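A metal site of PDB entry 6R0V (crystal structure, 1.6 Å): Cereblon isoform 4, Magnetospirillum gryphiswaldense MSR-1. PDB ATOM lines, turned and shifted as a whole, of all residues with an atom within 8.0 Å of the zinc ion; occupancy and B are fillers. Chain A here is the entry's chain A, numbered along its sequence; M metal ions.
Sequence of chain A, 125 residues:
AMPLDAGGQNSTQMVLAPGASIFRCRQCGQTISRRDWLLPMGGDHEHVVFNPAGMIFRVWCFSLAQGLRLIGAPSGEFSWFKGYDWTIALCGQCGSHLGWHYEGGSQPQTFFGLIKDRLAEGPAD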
ATOM      1  N   ARG A  24      19.684   9.529 -12.751  1.00  0.00           N
ATOM      2  CA  ARG A  24      20.439  10.056 -11.633  1.00  0.00           C
ATOM      3  C   ARG A  24      20.012   9.371 -10.327  1.00  0.00           C
ATOM      4  O   ARG A  24      18.921   8.855 -10.234  1.00  0.00           O
ATOM      5  CB  ARG A  24      20.199  11.553 -11.479  1.00  0.00           C
ATOM      6  CG  ARG A  24      20.580  12.337 -12.700  1.00  0.00           C
ATOM      7  CD  ARG A  24      20.565  13.848 -12.478  1.00  0.00           C
ATOM      8  NE  ARG A  24      21.224  14.503 -13.620  1.00  0.00           N
ATOM      9  CZ  ARG A  24      22.544  14.659 -13.767  1.00  0.00           C
ATOM     10  NH1 ARG A  24      23.390  14.338 -12.809  1.00  0.00           N
ATOM     11  NH2 ARG A  24      23.010  15.204 -14.857  1.00  0.00           N
ATOM     12  N   CYS A  25      20.886   9.402  -9.310  1.00  0.00           N
ATOM     13  CA  CYS A  25      20.491   8.943  -8.009  1.00  0.00           C
ATOM     14  C   CYS A  25      19.318   9.806  -7.485  1.00  0.00           C
ATOM     15  O   CYS A  25      19.425  11.036  -7.490  1.00  0.00           O
ATOM     16  CB  CYS A  25      21.654   9.063  -7.069  1.00  0.00           C
ATOM     17  SG  CYS A  25      21.246   8.644  -5.330  1.00  0.00           S
ATOM     18  N   ARG A  26      18.246   9.148  -7.054  1.00  0.00           N
ATOM     19  CA  ARG A  26      17.064   9.849  -6.550  1.00  0.00           C
ATOM     20  C   ARG A  26      17.337  10.677  -5.313  1.00  0.00           C
ATOM     21  O   ARG A  26      16.655  11.677  -5.055  1.00  0.00           O
ATOM     22  CB  ARG A  26      15.964   8.833  -6.265  1.00  0.00           C
ATOM     23  CG  ARG A  26      14.715   9.349  -5.661  1.00  0.00           C
ATOM     24  CD  ARG A  26      13.733   8.250  -5.445  1.00  0.00           C
ATOM     25  NE  ARG A  26      12.567   8.778  -4.741  1.00  0.00           N
ATOM     26  CZ  ARG A  26      11.476   8.079  -4.460  1.00  0.00           C
ATOM     27  NH1 ARG A  26      11.349   6.803  -4.879  1.00  0.00           N
ATOM     28  NH2 ARG A  26      10.525   8.643  -3.748  1.00  0.00           N
ATOM     29  N   GLN A  27      18.301  10.269  -4.511  1.00  0.00           N
ATOM     30  CA  GLN A  27      18.645  10.969  -3.262  1.00  0.00           C
ATOM     31  C   GLN A  27      19.522  12.189  -3.402  1.00  0.00           C
ATOM     32  O   GLN A  27      19.337  13.148  -2.669  1.00  0.00           O
ATOM     33  CB  GLN A  27      19.255  10.004  -2.248  1.00  0.00           C
ATOM     34  CG  GLN A  27      18.348   8.860  -1.898  1.00  0.00           C
ATOM     35  CD  GLN A  27      16.967   9.277  -1.411  1.00  0.00           C
ATOM     36  OE1 GLN A  27      16.816  10.247  -0.677  1.00  0.00           O
ATOM     37  NE2 GLN A  27      15.943   8.563  -1.866  1.00  0.00           N
ATOM     38  N   CYS A  28      20.451  12.195  -4.334  1.00  0.00           N
ATOM     39  CA  CYS A  28      21.467  13.255  -4.421  1.00  0.00           C
ATOM     40  C   CYS A  28      21.751  13.781  -5.822  1.00  0.00           C
ATOM     41  O   CYS A  28      22.424  14.788  -5.988  1.00  0.00           O
ATOM     42  CB  CYS A  28      22.760  12.770  -3.780  1.00  0.00           C
ATOM     43  SG  CYS A  28      23.656  11.615  -4.842  1.00  0.00           S
ATOM     44  N   GLY A  29      21.256  13.126  -6.874  1.00  0.00           N
ATOM     45  CA  GLY A  29      21.437  13.621  -8.201  1.00  0.00           C
ATOM     46  C   GLY A  29      22.675  13.172  -8.969  1.00  0.00           C
ATOM     47  O   GLY A  29      22.877  13.559 -10.134  1.00  0.00           O
ATOM     48  N   GLN A  30      23.540  12.380  -8.327  1.00  0.00           N
ATOM     49  CA  GLN A  30      24.714  11.825  -9.022  1.00  0.00           C
ATOM     50  C   GLN A  30      24.298  11.162 -10.328  1.00  0.00           C
ATOM     51  O   GLN A  30      23.351  10.413 -10.360  1.00  0.00           O
ATOM     52  CB  GLN A  30      25.393  10.791  -8.128  1.00  0.00           C
ATOM     53  CG  GLN A  30      26.553   9.991  -8.754  1.00  0.00           C
ATOM     54  CD  GLN A  30      27.700  10.894  -9.246  1.00  0.00           C
ATOM     55  OE1 GLN A  30      28.125  11.758  -8.511  1.00  0.00           O
ATOM     56  NE2 GLN A  30      28.188  10.704 -10.482  1.00  0.00           N
ATOM     57  N   THR A  31      25.033  11.447 -11.399  1.00  0.00           N
ATOM     58  CA  THR A  31      24.743  10.827 -12.688  1.00  0.00           C
ATOM     59  C   THR A  31      25.076   9.338 -12.623  1.00  0.00           C
ATOM     60  O   THR A  31      26.155   9.007 -12.152  1.00  0.00           O
ATOM     61  CB  THR A  31      25.606  11.452 -13.812  1.00  0.00           C
ATOM     62  OG1 THR A  31      25.662  12.884 -13.670  1.00  0.00           O
ATOM     63  CG2 THR A  31      25.044  11.069 -15.121  1.00  0.00           C
ATOM     64  N   ILE A  32      24.154   8.463 -13.028  1.00  0.00           N
ATOM     65  CA  ILE A  32      24.338   7.004 -12.889  1.00  0.00           C
ATOM     66  C   ILE A  32      24.305   6.282 -14.240  1.00  0.00           C
ATOM     67  O   ILE A  32      25.185   5.476 -14.525  1.00  0.00           O
ATOM     68  CB  ILE A  32      23.317   6.346 -11.931  1.00  0.00           C
ATOM     69  CG1 ILE A  32      23.338   6.984 -10.557  1.00  0.00           C
ATOM     70  CG2 ILE A  32      23.568   4.850 -11.839  1.00  0.00           C
ATOM     71  CD1 ILE A  32      24.602   6.834  -9.748  1.00  0.00           C
ATOM     72  N   GLY A  67      29.328   6.519 -11.551  1.00  0.00           N
ATOM     73  CA  GLY A  67      28.946   7.229 -10.322  1.00  0.00           C
ATOM     74  C   GLY A  67      28.664   6.293  -9.165  1.00  0.00           C
ATOM     75  O   GLY A  67      28.179   6.776  -8.148  1.00  0.00           O
ATOM     76  N   LEU A  68      28.919   4.992  -9.297  1.00  0.00           N
ATOM     77  CA  LEU A  68      28.647   4.013  -8.255  1.00  0.00           C
ATOM     78  C   LEU A  68      29.920   3.678  -7.527  1.00  0.00           C
ATOM     79  O   LEU A  68      30.992   4.063  -7.927  1.00  0.00           O
ATOM     80  CB  LEU A  68      28.047   2.729  -8.829  1.00  0.00           C
ATOM     81  CG  LEU A  68      26.742   2.937  -9.548  1.00  0.00           C
ATOM     82  CD1 LEU A  68      26.460   1.799 -10.507  1.00  0.00           C
ATOM     83  CD2 LEU A  68      25.585   3.170  -8.567  1.00  0.00           C
ATOM     84  N   LEU A  90      26.566   0.920  -4.605  1.00  0.00           N
ATOM     85  CA  LEU A  90      26.052   2.108  -3.934  1.00  0.00           C
ATOM     86  C   LEU A  90      26.268   3.330  -4.797  1.00  0.00           C
ATOM     87  O   LEU A  90      27.196   3.387  -5.594  1.00  0.00           O
ATOM     88  CB  LEU A  90      26.797   2.301  -2.612  1.00  0.00           C
ATOM     89  CG  LEU A  90      26.816   1.136  -1.615  1.00  0.00           C
ATOM     90  CD1 LEU A  90      27.559   1.616  -0.389  1.00  0.00           C
ATOM     91  CD2 LEU A  90      25.389   0.667  -1.313  1.00  0.00           C
ATOM     92  N   CYS A  91      25.433   4.329  -4.604  1.00  0.00           N
ATOM     93  CA  CYS A  91      25.751   5.671  -5.135  1.00  0.00           C
ATOM     94  C   CYS A  91      27.099   6.078  -4.552  1.00  0.00           C
ATOM     95  O   CYS A  91      27.295   6.072  -3.327  1.00  0.00           O
ATOM     96  CB  CYS A  91      24.706   6.671  -4.687  1.00  0.00           C
ATOM     97  SG  CYS A  91      24.995   8.361  -5.302  1.00  0.00           S
ATOM     98  N   GLY A  92      28.038   6.425  -5.449  1.00  0.00           N
ATOM     99  CA  GLY A  92      29.377   6.853  -5.038  1.00  0.00           C
ATOM    100  C   GLY A  92      29.393   8.186  -4.317  1.00  0.00           C
ATOM    101  O   GLY A  92      30.373   8.493  -3.615  1.00  0.00           O
ATOM    102  N   GLN A  93      28.338   8.970  -4.500  1.00  0.00           N
ATOM    103  CA  GLN A  93      28.231  10.250  -3.830  1.00  0.00           C
ATOM    104  C   GLN A  93      27.613  10.147  -2.421  1.00  0.00           C
ATOM    105  O   GLN A  93      28.204  10.537  -1.441  1.00  0.00           O
ATOM    106  CB  GLN A  93      27.477  11.210  -4.751  1.00  0.00           C
ATOM    107  CG  GLN A  93      27.334  12.626  -4.243  1.00  0.00           C
ATOM    108  CD  GLN A  93      27.091  13.606  -5.370  1.00  0.00           C
ATOM    109  OE1 GLN A  93      28.045  14.206  -5.874  1.00  0.00           O
ATOM    110  NE2 GLN A  93      25.834  13.731  -5.797  1.00  0.00           N
ATOM    111  N   CYS A  94      26.414   9.572  -2.342  1.00  0.00           N
ATOM    112  CA  CYS A  94      25.638   9.587  -1.097  1.00  0.00           C
ATOM    113  C   CYS A  94      25.503   8.263  -0.367  1.00  0.00           C
ATOM    114  O   CYS A  94      25.025   8.271   0.764  1.00  0.00           O
ATOM    115  CB  CYS A  94      24.269  10.146  -1.349  1.00  0.00           C
ATOM    116  SG  CYS A  94      23.033   9.033  -2.075  1.00  0.00           S
ATOM    117  N   GLY A  95      25.907   7.148  -1.013  1.00  0.00           N
ATOM    118  CA  GLY A  95      25.851   5.852  -0.376  1.00  0.00           C
ATOM    119  C   GLY A  95      24.530   5.119  -0.515  1.00  0.00           C
ATOM    120  O   GLY A  95      24.396   4.013  -0.001  1.00  0.00           O
ATOM    121  N   SER A  96      23.527   5.711  -1.172  1.00  0.00           N
ATOM    122  CA  SER A  96      22.230   5.025  -1.434  1.00  0.00           C
ATOM    123  C   SER A  96      22.471   3.707  -2.150  1.00  0.00           C
ATOM    124  O   SER A  96      23.278   3.629  -3.055  1.00  0.00           O
ATOM    125  CB  SER A  96      21.288   5.925  -2.216  1.00  0.00           C
ATOM    126  OG  SER A  96      20.041   5.275  -2.481  1.00  0.00           O
ATOM    127  N   HIS A  97      21.796   2.649  -1.719  1.00  0.00           N
ATOM    128  CA  HIS A  97      21.949   1.378  -2.405  1.00  0.00           C
ATOM    129  C   HIS A  97      21.126   1.381  -3.686  1.00  0.00           C
ATOM    130  O   HIS A  97      19.909   1.301  -3.643  1.00  0.00           O
ATOM    131  CB  HIS A  97      21.524   0.223  -1.504  1.00  0.00           C
ATOM    132  CG  HIS A  97      21.621  -1.083  -2.179  1.00  0.00           C
ATOM    133  ND1 HIS A  97      20.901  -2.183  -1.766  1.00  0.00           N
ATOM    134  CD2 HIS A  97      22.350  -1.488  -3.257  1.00  0.00           C
ATOM    135  CE1 HIS A  97      21.188  -3.201  -2.544  1.00  0.00           C
ATOM    136  NE2 HIS A  97      22.035  -2.789  -3.490  1.00  0.00           N
ATOM    137  N   LEU A  98      21.785   1.501  -4.828  1.00  0.00           N
ATOM    138  CA  LEU A  98      21.102   1.654  -6.116  1.00  0.00           C
ATOM    139  C   LEU A  98      20.902   0.353  -6.902  1.00  0.00           C
ATOM    140  O   LEU A  98      20.057   0.284  -7.782  1.00  0.00           O
ATOM    141  CB  LEU A  98      21.847   2.676  -6.993  1.00  0.00           C
ATOM    142  CG  LEU A  98      21.902   4.099  -6.412  1.00  0.00           C
ATOM    143  CD1 LEU A  98      22.470   5.049  -7.417  1.00  0.00           C
ATOM    144  CD2 LEU A  98      20.533   4.600  -5.984  1.00  0.00           C
ATOM    145  N   ARG A 118      14.774   3.856  -7.288  1.00  0.00           N
ATOM    146  CA  ARG A 118      15.835   4.578  -6.592  1.00  0.00           C
ATOM    147  C   ARG A 118      16.618   5.498  -7.521  1.00  0.00           C
ATOM    148  O   ARG A 118      17.585   6.123  -7.089  1.00  0.00           O
ATOM    149  CB  ARG A 118      16.755   3.598  -5.870  1.00  0.00           C
ATOM    150  CG  ARG A 118      15.971   2.796  -4.875  1.00  0.00           C
ATOM    151  CD  ARG A 118      16.832   1.930  -3.968  1.00  0.00           C
ATOM    152  NE  ARG A 118      16.017   1.057  -3.141  1.00  0.00           N
ATOM    153  CZ  ARG A 118      16.496   0.218  -2.223  1.00  0.00           C
ATOM    154  NH1 ARG A 118      17.822   0.125  -2.010  1.00  0.00           N
ATOM    155  NH2 ARG A 118      15.673  -0.525  -1.498  1.00  0.00           N
HETATM  156 ZN    ZN M   1      23.165   9.407  -4.331  1.00  0.00          ZN
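N of Ser 96 lies close to SG of Cys 94 (3.5 Å).
The side-chain sulfur (SG) of Cys 25 lies close to the backbone NH (N) of Gln 27, at 3.5 Å.
The backbone NH (N) of Cys 25 sits at hydrogen-bond distance from the backbone carbonyl oxygen (O) of Gln 30, 2.9 Å away.
SG of Cys 28 lies close to N of Gln 30 (3.6 Å).
The side-chain sulfur (SG) of Cys 28 sits close to the side-chain amide nitrogen (NE2) of Gln 93.
N of Cys 91 sits at hydrogen-bond distance from O of Ser 96 (2.7 Å).
The side-chain sulfur (SG) of Cys 91 lies close to the backbone NH (N) of Gln 93, 3.5 Å away.
Of the 21 residues printed, 4 come within 4 Å of the zinc ion.
The zinc ion is bound by SG of Cys 94 (2.3 Å), SG of Cys 25 (2.3 Å), SG of Cys 28 (2.3 Å) and SG of Cys 91 (2.3 Å).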
